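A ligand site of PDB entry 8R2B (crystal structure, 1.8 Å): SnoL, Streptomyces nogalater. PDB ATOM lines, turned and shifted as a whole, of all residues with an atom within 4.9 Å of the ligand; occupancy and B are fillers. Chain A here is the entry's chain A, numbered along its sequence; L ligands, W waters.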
ATOM      1  N   MET A  22     -11.146  41.975  22.187  1.00  0.00           N
ATOM      2  CA  MET A  22     -10.624  40.654  22.025  1.00  0.00           C
ATOM      3  C   MET A  22     -11.699  39.744  21.463  1.00  0.00           C
ATOM      4  O   MET A  22     -11.384  38.901  20.621  1.00  0.00           O
ATOM      5  CB  MET A  22     -10.128  40.079  23.373  1.00  0.00           C
ATOM      6  CG  MET A  22      -8.973  40.873  24.002  1.00  0.00           C
ATOM      7  SD  MET A  22      -8.713  40.429  25.752  1.00  0.00           S
ATOM      8  CE  MET A  22      -8.334  41.981  26.435  1.00  0.00           C
ATOM      9  N   TRP A  26     -11.567  37.603  17.857  1.00  0.00           N
ATOM     10  CA  TRP A  26     -11.924  36.207  17.668  1.00  0.00           C
ATOM     11  C   TRP A  26     -12.983  36.028  16.580  1.00  0.00           C
ATOM     12  O   TRP A  26     -12.981  35.084  15.803  1.00  0.00           O
ATOM     13  CB  TRP A  26     -12.547  35.610  18.940  1.00  0.00           C
ATOM     14  CG  TRP A  26     -11.561  34.942  19.909  1.00  0.00           C
ATOM     15  CD1 TRP A  26     -11.188  35.396  21.103  1.00  0.00           C
ATOM     16  CD2 TRP A  26     -10.901  33.740  19.705  1.00  0.00           C
ATOM     17  NE1 TRP A  26     -10.299  34.531  21.688  1.00  0.00           N
ATOM     18  CE2 TRP A  26     -10.104  33.496  20.834  1.00  0.00           C
ATOM     19  CE3 TRP A  26     -10.898  32.812  18.680  1.00  0.00           C
ATOM     20  CZ2 TRP A  26      -9.341  32.380  20.966  1.00  0.00           C
ATOM     21  CZ3 TRP A  26     -10.122  31.684  18.824  1.00  0.00           C
ATOM     22  CH2 TRP A  26      -9.352  31.484  19.965  1.00  0.00           C
ATOM     23  N   VAL A  34      -6.060  39.160  19.430  1.00  0.00           N
ATOM     24  CA  VAL A  34      -6.274  38.825  20.827  1.00  0.00           C
ATOM     25  C   VAL A  34      -4.934  39.048  21.531  1.00  0.00           C
ATOM     26  O   VAL A  34      -4.872  39.732  22.533  1.00  0.00           O
ATOM     27  CB  VAL A  34      -6.779  37.384  20.990  1.00  0.00           C
ATOM     28  CG1 VAL A  34      -6.975  37.116  22.473  1.00  0.00           C
ATOM     29  CG2 VAL A  34      -8.131  37.165  20.237  1.00  0.00           C
ATOM     30  N   TRP A  38      -1.980  41.293  25.317  1.00  0.00           N
ATOM     31  CA  TRP A  38      -1.193  40.677  26.375  1.00  0.00           C
ATOM     32  C   TRP A  38       0.013  41.507  26.795  1.00  0.00           C
ATOM     33  O   TRP A  38       0.721  42.079  25.948  1.00  0.00           O
ATOM     34  CB  TRP A  38      -0.681  39.334  25.922  1.00  0.00           C
ATOM     35  CG  TRP A  38      -1.725  38.350  25.667  1.00  0.00           C
ATOM     36  CD1 TRP A  38      -3.060  38.487  25.929  1.00  0.00           C
ATOM     37  CD2 TRP A  38      -1.546  37.054  25.181  1.00  0.00           C
ATOM     38  NE1 TRP A  38      -3.712  37.369  25.556  1.00  0.00           N
ATOM     39  CE2 TRP A  38      -2.810  36.457  25.116  1.00  0.00           C
ATOM     40  CE3 TRP A  38      -0.454  36.344  24.718  1.00  0.00           C
ATOM     41  CZ2 TRP A  38      -3.019  35.195  24.657  1.00  0.00           C
ATOM     42  CZ3 TRP A  38      -0.654  35.091  24.266  1.00  0.00           C
ATOM     43  CH2 TRP A  38      -1.943  34.508  24.218  1.00  0.00           C
ATOM     44  N   HIS A  44      -0.641  32.704  31.825  1.00  0.00           N
ATOM     45  CA  HIS A  44      -1.883  32.017  31.542  1.00  0.00           C
ATOM     46  C   HIS A  44      -1.882  30.729  32.314  1.00  0.00           C
ATOM     47  O   HIS A  44      -0.883  30.063  32.330  1.00  0.00           O
ATOM     48  CB  HIS A  44      -1.959  31.580  30.096  1.00  0.00           C
ATOM     49  CG  HIS A  44      -1.876  32.697  29.140  1.00  0.00           C
ATOM     50  ND1 HIS A  44      -2.997  33.373  28.723  1.00  0.00           N
ATOM     51  CD2 HIS A  44      -0.832  33.267  28.505  1.00  0.00           C
ATOM     52  CE1 HIS A  44      -2.651  34.320  27.886  1.00  0.00           C
ATOM     53  NE2 HIS A  44      -1.347  34.228  27.671  1.00  0.00           N
ATOM     54  N   ASP A  46      -3.557  26.985  33.075  1.00  0.00           N
ATOM     55  CA  ASP A  46      -4.341  25.904  32.537  1.00  0.00           C
ATOM     56  C   ASP A  46      -5.371  25.444  33.509  1.00  0.00           C
ATOM     57  O   ASP A  46      -5.540  25.982  34.610  1.00  0.00           O
ATOM     58  CB  ASP A  46      -3.466  24.772  32.126  1.00  0.00           C
ATOM     59  CG  ASP A  46      -2.820  24.036  33.277  1.00  0.00           C
ATOM     60  OD1 ASP A  46      -3.252  24.068  34.466  1.00  0.00           O
ATOM     61  OD2 ASP A  46      -1.856  23.346  32.875  1.00  0.00           O
ATOM     62  N   ASP A  47      -6.084  24.429  33.075  1.00  0.00           N
ATOM     63  CA  ASP A  47      -7.169  23.871  33.870  1.00  0.00           C
ATOM     64  C   ASP A  47      -6.842  23.404  35.286  1.00  0.00           C
ATOM     65  O   ASP A  47      -7.743  23.181  36.065  1.00  0.00           O
ATOM     66  CB  ASP A  47      -7.846  22.697  33.092  1.00  0.00           C
ATOM     67  CG  ASP A  47      -6.904  21.468  32.877  1.00  0.00           C
ATOM     68  OD1 ASP A  47      -6.071  21.504  31.934  1.00  0.00           O
ATOM     69  OD2 ASP A  47      -7.057  20.451  33.595  1.00  0.00           O
ATOM     70  N   VAL A  52       0.843  28.125  31.671  1.00  0.00           N
ATOM     71  CA  VAL A  52       1.032  27.652  30.279  1.00  0.00           C
ATOM     72  C   VAL A  52       1.740  28.710  29.494  1.00  0.00           C
ATOM     73  O   VAL A  52       1.417  29.907  29.612  1.00  0.00           O
ATOM     74  CB  VAL A  52      -0.321  27.483  29.572  1.00  0.00           C
ATOM     75  CG1 VAL A  52      -0.115  26.895  28.181  1.00  0.00           C
ATOM     76  CG2 VAL A  52      -1.222  26.600  30.373  1.00  0.00           C
ATOM     77  N   VAL A  57      -0.308  28.782  24.331  1.00  0.00           N
ATOM     78  CA  VAL A  57      -1.649  29.313  24.283  1.00  0.00           C
ATOM     79  C   VAL A  57      -1.936  29.734  22.840  1.00  0.00           C
ATOM     80  O   VAL A  57      -2.982  29.366  22.304  1.00  0.00           O
ATOM     81  CB  VAL A  57      -1.860  30.418  25.311  1.00  0.00           C
ATOM     82  CG1 VAL A  57      -3.250  31.062  25.157  1.00  0.00           C
ATOM     83  CG2 VAL A  57      -1.711  29.799  26.715  1.00  0.00           C
ATOM     84  N   ARG A  60      -2.756  26.762  20.703  1.00  0.00           N
ATOM     85  CA  ARG A  60      -4.104  26.264  20.883  1.00  0.00           C
ATOM     86  C   ARG A  60      -5.094  27.198  20.245  1.00  0.00           C
ATOM     87  O   ARG A  60      -6.030  26.721  19.696  1.00  0.00           O
ATOM     88  CB  ARG A  60      -4.411  26.135  22.389  1.00  0.00           C
ATOM     89  CG  ARG A  60      -3.598  25.057  23.079  1.00  0.00           C
ATOM     90  CD  ARG A  60      -3.571  25.247  24.590  1.00  0.00           C
ATOM     91  NE  ARG A  60      -2.693  24.262  25.192  1.00  0.00           N
ATOM     92  CZ  ARG A  60      -2.724  23.849  26.464  1.00  0.00           C
ATOM     93  NH1 ARG A  60      -3.587  24.317  27.338  1.00  0.00           N
ATOM     94  NH2 ARG A  60      -1.837  22.949  26.856  1.00  0.00           N
ATOM     95  N   MET A  61      -4.931  28.507  20.362  1.00  0.00           N
ATOM     96  CA  MET A  61      -5.871  29.421  19.755  1.00  0.00           C
ATOM     97  C   MET A  61      -5.868  29.287  18.236  1.00  0.00           C
ATOM     98  O   MET A  61      -6.912  29.287  17.608  1.00  0.00           O
ATOM     99  CB  MET A  61      -5.548  30.859  20.118  1.00  0.00           C
ATOM    100  CG  MET A  61      -5.831  31.153  21.596  1.00  0.00           C
ATOM    101  SD  MET A  61      -4.968  32.616  22.142  1.00  0.00           S
ATOM    102  CE  MET A  61      -6.151  33.790  21.722  1.00  0.00           C
ATOM    103  N   ALA A  64      -7.840  26.281  17.105  1.00  0.00           N
ATOM    104  CA  ALA A  64      -9.278  26.460  17.186  1.00  0.00           C
ATOM    105  C   ALA A  64      -9.799  27.228  16.004  1.00  0.00           C
ATOM    106  O   ALA A  64     -10.824  26.856  15.473  1.00  0.00           O
ATOM    107  CB  ALA A  64      -9.653  27.170  18.475  1.00  0.00           C
ATOM    108  N   LEU A  71     -16.501  30.031  13.679  1.00  0.00           N
ATOM    109  CA  LEU A  71     -16.884  30.242  15.069  1.00  0.00           C
ATOM    110  C   LEU A  71     -17.407  31.643  15.298  1.00  0.00           C
ATOM    111  O   LEU A  71     -17.014  32.609  14.628  1.00  0.00           O
ATOM    112  CB  LEU A  71     -15.719  29.879  16.021  1.00  0.00           C
ATOM    113  CG  LEU A  71     -14.552  30.826  16.122  1.00  0.00           C
ATOM    114  CD1 LEU A  71     -14.783  31.966  17.104  1.00  0.00           C
ATOM    115  CD2 LEU A  71     -13.287  30.065  16.537  1.00  0.00           C
ATOM    116  N   LEU A  73     -18.673  34.101  18.765  1.00  0.00           N
ATOM    117  CA  LEU A  73     -18.713  34.223  20.215  1.00  0.00           C
ATOM    118  C   LEU A  73     -19.722  35.277  20.564  1.00  0.00           C
ATOM    119  O   LEU A  73     -19.710  36.344  20.023  1.00  0.00           O
ATOM    120  CB  LEU A  73     -17.372  34.713  20.759  1.00  0.00           C
ATOM    121  CG  LEU A  73     -16.160  33.848  20.401  1.00  0.00           C
ATOM    122  CD1 LEU A  73     -14.947  34.395  21.171  1.00  0.00           C
ATOM    123  CD2 LEU A  73     -16.411  32.409  20.812  1.00  0.00           C
ATOM    124  N   ILE A  89     -19.184  33.535  27.977  1.00  0.00           N
ATOM    125  CA  ILE A  89     -19.232  33.611  26.535  1.00  0.00           C
ATOM    126  C   ILE A  89     -19.759  32.303  25.988  1.00  0.00           C
ATOM    127  O   ILE A  89     -19.440  31.201  26.520  1.00  0.00           O
ATOM    128  CB  ILE A  89     -17.822  33.782  25.988  1.00  0.00           C
ATOM    129  CG1 ILE A  89     -17.206  35.033  26.589  1.00  0.00           C
ATOM    130  CG2 ILE A  89     -17.843  33.835  24.493  1.00  0.00           C
ATOM    131  CD1 ILE A  89     -15.749  35.253  26.218  1.00  0.00           C
ATOM    132  N   CYS A  91     -19.754  30.050  22.460  1.00  0.00           N
ATOM    133  CA  CYS A  91     -19.162  29.872  21.159  1.00  0.00           C
ATOM    134  C   CYS A  91     -19.971  28.851  20.399  1.00  0.00           C
ATOM    135  O   CYS A  91     -20.316  27.810  20.948  1.00  0.00           O
ATOM    136  CB  CYS A  91     -17.757  29.357  21.323  1.00  0.00           C
ATOM    137  SG  CYS A  91     -16.912  29.042  19.740  1.00  0.00           S
ATOM    138  N   PHE A  99      -9.144  19.013  16.372  1.00  0.00           N
ATOM    139  CA  PHE A  99      -8.825  19.914  17.510  1.00  0.00           C
ATOM    140  C   PHE A  99      -8.465  19.031  18.715  1.00  0.00           C
ATOM    141  O   PHE A  99      -9.241  18.168  19.109  1.00  0.00           O
ATOM    142  CB  PHE A  99     -10.019  20.827  17.826  1.00  0.00           C
ATOM    143  CG  PHE A  99      -9.797  21.785  18.968  1.00  0.00           C
ATOM    144  CD1 PHE A  99      -8.948  22.853  18.831  1.00  0.00           C
ATOM    145  CD2 PHE A  99     -10.491  21.628  20.157  1.00  0.00           C
ATOM    146  CE1 PHE A  99      -8.732  23.753  19.872  1.00  0.00           C
ATOM    147  CE2 PHE A  99     -10.301  22.492  21.206  1.00  0.00           C
ATOM    148  CZ  PHE A  99      -9.403  23.562  21.058  1.00  0.00           C
ATOM    149  N   MET A 100      -7.275  19.222  19.246  1.00  0.00           N
ATOM    150  CA  MET A 100      -6.821  18.435  20.440  1.00  0.00           C
ATOM    151  C   MET A 100      -7.076  17.002  20.262  1.00  0.00           C
ATOM    152  O   MET A 100      -7.729  16.340  21.087  1.00  0.00           O
ATOM    153  CB  MET A 100      -7.543  18.941  21.687  1.00  0.00           C
ATOM    154  CG  MET A 100      -7.365  20.428  21.873  1.00  0.00           C
ATOM    155  SD  MET A 100      -5.649  20.771  22.145  1.00  0.00           S
ATOM    156  CE  MET A 100      -5.423  22.335  21.386  1.00  0.00           C
ATOM    157  N   TRP A 111     -20.579  25.672  22.966  1.00  0.00           N
ATOM    158  CA  TRP A 111     -20.138  25.572  24.344  1.00  0.00           C
ATOM    159  C   TRP A 111     -20.118  26.942  24.973  1.00  0.00           C
ATOM    160  O   TRP A 111     -19.939  27.935  24.266  1.00  0.00           O
ATOM    161  CB  TRP A 111     -18.767  24.912  24.471  1.00  0.00           C
ATOM    162  CG  TRP A 111     -17.635  25.570  23.782  1.00  0.00           C
ATOM    163  CD1 TRP A 111     -16.886  26.506  24.281  1.00  0.00           C
ATOM    164  CD2 TRP A 111     -17.081  25.236  22.507  1.00  0.00           C
ATOM    165  NE1 TRP A 111     -15.899  26.891  23.360  1.00  0.00           N
ATOM    166  CE2 TRP A 111     -16.007  26.116  22.265  1.00  0.00           C
ATOM    167  CE3 TRP A 111     -17.410  24.322  21.518  1.00  0.00           C
ATOM    168  CZ2 TRP A 111     -15.246  26.099  21.099  1.00  0.00           C
ATOM    169  CZ3 TRP A 111     -16.622  24.301  20.349  1.00  0.00           C
ATOM    170  CH2 TRP A 111     -15.577  25.194  20.160  1.00  0.00           C
ATOM    171  N   TYR A 113     -18.430  29.322  28.298  1.00  0.00           N
ATOM    172  CA  TYR A 113     -17.263  29.347  29.115  1.00  0.00           C
ATOM    173  C   TYR A 113     -17.038  30.610  29.821  1.00  0.00           C
ATOM    174  O   TYR A 113     -17.638  31.603  29.486  1.00  0.00           O
ATOM    175  CB  TYR A 113     -16.032  29.018  28.307  1.00  0.00           C
ATOM    176  CG  TYR A 113     -15.671  29.920  27.162  1.00  0.00           C
ATOM    177  CD1 TYR A 113     -14.640  30.819  27.273  1.00  0.00           C
ATOM    178  CD2 TYR A 113     -16.300  29.794  25.954  1.00  0.00           C
ATOM    179  CE1 TYR A 113     -14.245  31.622  26.206  1.00  0.00           C
ATOM    180  CE2 TYR A 113     -15.932  30.581  24.853  1.00  0.00           C
ATOM    181  CZ  TYR A 113     -14.894  31.479  24.970  1.00  0.00           C
ATOM    182  OH  TYR A 113     -14.498  32.281  23.918  1.00  0.00           O
ATOM    183  N   GLU A 115     -14.101  33.547  30.859  1.00  0.00           N
ATOM    184  CA  GLU A 115     -12.803  34.094  30.671  1.00  0.00           C
ATOM    185  C   GLU A 115     -12.630  35.081  31.782  1.00  0.00           C
ATOM    186  O   GLU A 115     -13.445  35.996  31.917  1.00  0.00           O
ATOM    187  CB  GLU A 115     -12.692  34.850  29.349  1.00  0.00           C
ATOM    188  CG  GLU A 115     -12.547  33.963  28.150  1.00  0.00           C
ATOM    189  CD  GLU A 115     -11.270  33.149  28.165  1.00  0.00           C
ATOM    190  OE1 GLU A 115     -10.295  33.630  28.733  1.00  0.00           O
ATOM    191  OE2 GLU A 115     -11.272  32.037  27.652  1.00  0.00           O
ATOM    192  N   LEU A 117      -9.834  37.954  33.114  1.00  0.00           N
ATOM    193  CA  LEU A 117      -8.639  38.653  32.798  1.00  0.00           C
ATOM    194  C   LEU A 117      -8.274  39.690  33.867  1.00  0.00           C
ATOM    195  O   LEU A 117      -9.146  40.424  34.326  1.00  0.00           O
ATOM    196  CB  LEU A 117      -8.848  39.352  31.452  1.00  0.00           C
ATOM    197  CG  LEU A 117      -9.140  38.333  30.364  1.00  0.00           C
ATOM    198  CD1 LEU A 117     -10.157  38.884  29.422  1.00  0.00           C
ATOM    199  CD2 LEU A 117      -7.940  37.804  29.657  1.00  0.00           C
ATOM    200  N   HIS A 128      -4.424  35.497  33.227  1.00  0.00           N
ATOM    201  CA  HIS A 128      -5.551  35.027  32.467  1.00  0.00           C
ATOM    202  C   HIS A 128      -5.928  33.638  32.912  1.00  0.00           C
ATOM    203  O   HIS A 128      -5.097  32.745  32.997  1.00  0.00           O
ATOM    204  CB  HIS A 128      -5.174  35.011  30.971  1.00  0.00           C
ATOM    205  CG  HIS A 128      -6.133  34.251  30.134  1.00  0.00           C
ATOM    206  ND1 HIS A 128      -5.742  33.264  29.280  1.00  0.00           N
ATOM    207  CD2 HIS A 128      -7.474  34.327  30.046  1.00  0.00           C
ATOM    208  CE1 HIS A 128      -6.811  32.739  28.704  1.00  0.00           C
ATOM    209  NE2 HIS A 128      -7.871  33.393  29.148  1.00  0.00           N
ATOM    210  N   ASP A 130      -9.327  30.632  32.465  1.00  0.00           N
ATOM    211  CA  ASP A 130     -10.532  30.194  31.740  1.00  0.00           C
ATOM    212  C   ASP A 130     -11.219  29.072  32.550  1.00  0.00           C
ATOM    213  O   ASP A 130     -10.575  28.365  33.319  1.00  0.00           O
ATOM    214  CB  ASP A 130     -10.293  29.498  30.428  1.00  0.00           C
ATOM    215  CG  ASP A 130      -9.104  30.008  29.608  1.00  0.00           C
ATOM    216  OD1 ASP A 130      -9.205  30.841  28.648  1.00  0.00           O
ATOM    217  OD2 ASP A 130      -8.046  29.499  29.824  1.00  0.00           O
ATOM    218  N   PHE A 132     -13.780  26.052  31.064  1.00  0.00           N
ATOM    219  CA  PHE A 132     -14.528  25.507  29.949  1.00  0.00           C
ATOM    220  C   PHE A 132     -15.294  24.209  30.232  1.00  0.00           C
ATOM    221  O   PHE A 132     -14.820  23.351  30.903  1.00  0.00           O
ATOM    222  CB  PHE A 132     -13.563  25.202  28.788  1.00  0.00           C
ATOM    223  CG  PHE A 132     -13.081  26.408  28.021  1.00  0.00           C
ATOM    224  CD1 PHE A 132     -11.998  27.107  28.432  1.00  0.00           C
ATOM    225  CD2 PHE A 132     -13.696  26.805  26.882  1.00  0.00           C
ATOM    226  CE1 PHE A 132     -11.537  28.194  27.726  1.00  0.00           C
ATOM    227  CE2 PHE A 132     -13.269  27.897  26.186  1.00  0.00           C
ATOM    228  CZ  PHE A 132     -12.185  28.596  26.612  1.00  0.00           C
ATOM    229  N   PHE A 134     -16.218  21.675  27.894  1.00  0.00           N
ATOM    230  CA  PHE A 134     -16.008  21.167  26.563  1.00  0.00           C
ATOM    231  C   PHE A 134     -16.753  19.869  26.291  1.00  0.00           C
ATOM    232  O   PHE A 134     -16.546  19.251  25.282  1.00  0.00           O
ATOM    233  CB  PHE A 134     -14.517  20.911  26.340  1.00  0.00           C
ATOM    234  CG  PHE A 134     -13.752  22.092  25.874  1.00  0.00           C
ATOM    235  CD1 PHE A 134     -14.195  22.853  24.849  1.00  0.00           C
ATOM    236  CD2 PHE A 134     -12.572  22.416  26.447  1.00  0.00           C
ATOM    237  CE1 PHE A 134     -13.489  23.922  24.412  1.00  0.00           C
ATOM    238  CE2 PHE A 134     -11.844  23.492  26.002  1.00  0.00           C
ATOM    239  CZ  PHE A 134     -12.321  24.257  25.001  1.00  0.00           C
HETATM  240  C1  LIG L   1      -4.643  27.788  27.503  1.00  0.00           C
HETATM  241  O1  LIG L   1      -5.304  26.655  26.982  1.00  0.00           O
HETATM  242  C2  LIG L   1      -6.663  26.997  26.927  1.00  0.00           C
HETATM  243  C3  LIG L   1      -7.376  25.874  27.547  1.00  0.00           C
HETATM  244  C4  LIG L   1      -8.805  26.260  27.820  1.00  0.00           C
HETATM  245  O2  LIG L   1      -6.789  25.610  28.843  1.00  0.00           O
HETATM  246  C5  LIG L   1      -7.239  24.653  26.783  1.00  0.00           C
HETATM  247  O3  LIG L   1      -8.125  23.623  27.301  1.00  0.00           O
HETATM  248  C6  LIG L   1      -7.633  24.888  25.363  1.00  0.00           C
HETATM  249  C7  LIG L   1      -7.408  23.561  24.581  1.00  0.00           C
HETATM  250  O4  LIG L   1      -6.851  25.874  24.881  1.00  0.00           O
HETATM  251  C8  LIG L   1      -6.954  27.134  25.473  1.00  0.00           C
HETATM  252  O5  LIG L   1      -8.213  27.735  25.342  1.00  0.00           O
HETATM  253  C9  LIG L   1      -8.514  28.226  23.996  1.00  0.00           C
HETATM  254  C10 LIG L   1      -9.335  27.154  23.348  1.00  0.00           C
HETATM  255  C11 LIG L   1     -10.438  27.739  22.436  1.00  0.00           C
HETATM  256  C12 LIG L   1     -11.255  26.615  21.772  1.00  0.00           C
HETATM  257  O6  LIG L   1      -9.810  28.523  21.356  1.00  0.00           O
HETATM  258  C13 LIG L   1      -9.116  29.511  24.134  1.00  0.00           C
HETATM  259  C14 LIG L   1      -8.377  30.572  24.611  1.00  0.00           C
HETATM  260  O7  LIG L   1      -7.079  30.356  24.874  1.00  0.00           O
HETATM  261  C15 LIG L   1      -8.882  31.860  24.776  1.00  0.00           C
HETATM  262  C16 LIG L   1      -8.052  32.885  25.215  1.00  0.00           C
HETATM  263  O8  LIG L   1      -6.848  32.665  25.480  1.00  0.00           O
HETATM  264  C17 LIG L   1      -8.571  34.125  25.388  1.00  0.00           C
HETATM  265  C18 LIG L   1      -7.768  35.154  25.843  1.00  0.00           C
HETATM  266  O9  LIG L   1      -6.490  34.853  26.034  1.00  0.00           O
HETATM  267  C19 LIG L   1      -8.236  36.436  26.027  1.00  0.00           C
HETATM  268  C20 LIG L   1      -9.581  36.669  25.775  1.00  0.00           C
HETATM  269  C21 LIG L   1     -10.422  35.687  25.296  1.00  0.00           C
HETATM  270  C22 LIG L   1      -9.912  34.388  25.122  1.00  0.00           C
HETATM  271  C23 LIG L   1     -10.754  33.375  24.685  1.00  0.00           C
HETATM  272  O10 LIG L   1     -11.956  33.594  24.449  1.00  0.00           O
HETATM  273  C24 LIG L   1     -10.208  32.090  24.501  1.00  0.00           C
HETATM  274  C25 LIG L   1     -10.994  31.048  24.023  1.00  0.00           C
HETATM  275  C26 LIG L   1     -10.500  29.763  23.808  1.00  0.00           C
HETATM  276  C27 LIG L   1     -11.332  28.709  23.319  1.00  0.00           C
HETATM  277  C28 LIG L   1     -12.405  29.154  22.512  1.00  0.00           C
HETATM  278  O11 LIG L   1     -13.588  28.860  22.779  1.00  0.00           O
HETATM  279  O12 LIG L   1     -12.035  29.871  21.408  1.00  0.00           O
HETATM  280  C29 LIG L   1     -13.115  30.447  20.686  1.00  0.00           C
HETATM  281  O   HOH W   1      -5.944  38.786  25.335  1.00  0.00           O
HETATM  282  O   HOH W   2      -5.441  23.245  29.925  1.00  0.00           O
HETATM  283  O   HOH W   3      -9.982  23.107  29.953  1.00  0.00           O
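The side-chain hydroxyl of Tyr 113 is in hydrogen-bond range of an oxygen (O10) of the ligand, 2.9 Å away. An oxygen (O1) of the ligand is in hydrogen-bond range of the guanidinium group (NH1) of Arg 60. O11 of the ligand lies within hydrogen-bond range of NE1 of Trp 111 (3.1 Å). O10 of the ligand sits close to NE1 of Trp 26 (3.4 Å).
N of Tyr 113 is in hydrogen-bond range of O of Ile 89. N of Cys 91 sits at hydrogen-bond distance from O of Trp 111 (2.8 Å). NE2 of His 128 is in hydrogen-bond range of OE1 of Glu 115, at 2.5 Å. A ring nitrogen (NE2) of His 128 is in hydrogen-bond range of the side-chain carboxylate (OD1) of Asp 130. ND1 of His 44 sits at hydrogen-bond distance from ND1 of His 128, at 2.8 Å. OE2 of Glu 115 sits close to OD1 of Asp 130 (2.6 Å).
Merely in contact with the ligand: Ala 64 (3.2 Å), His 128 (3.2 Å), Glu 115 (3.3 Å), Phe 132 (3.3 Å), Met 61 (3.6 Å), Phe 99 (3.6 Å), Val 57 (3.6 Å), Trp 38 (3.7 Å), Val 34 (3.8 Å), Leu 73 (3.8 Å), Met 22 (3.9 Å), Asp 130 (3.9 Å), Leu 117 (3.9 Å), Phe 134 (3.9 Å) and Met 100 (3.96 Å). Hydrophobic or aromatic side chains that line the ligand: Met 22, Trp 26, Val 34, Trp 38, Val 57, Met 61, Ala 64, Leu 73, Phe 99, Met 100, Trp 111, Tyr 113, Leu 117, His 128, Phe 132 and Phe 134.
Water W2 lies within hydrogen-bond range of the side-chain carboxylate of Asp 47 (2.7 Å), an oxygen (O2) of the ligand (2.9 Å) and the guanidinium group of Arg 60 (3.4 Å). Water W1 lies within hydrogen-bond range of the indole nitrogen (NE1) of Trp 38 (2.7 Å), the backbone carbonyl oxygen (O) of Val 34 (3.1 Å) and the side-chain sulfur (SD) of Met 22 (3.2 Å).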
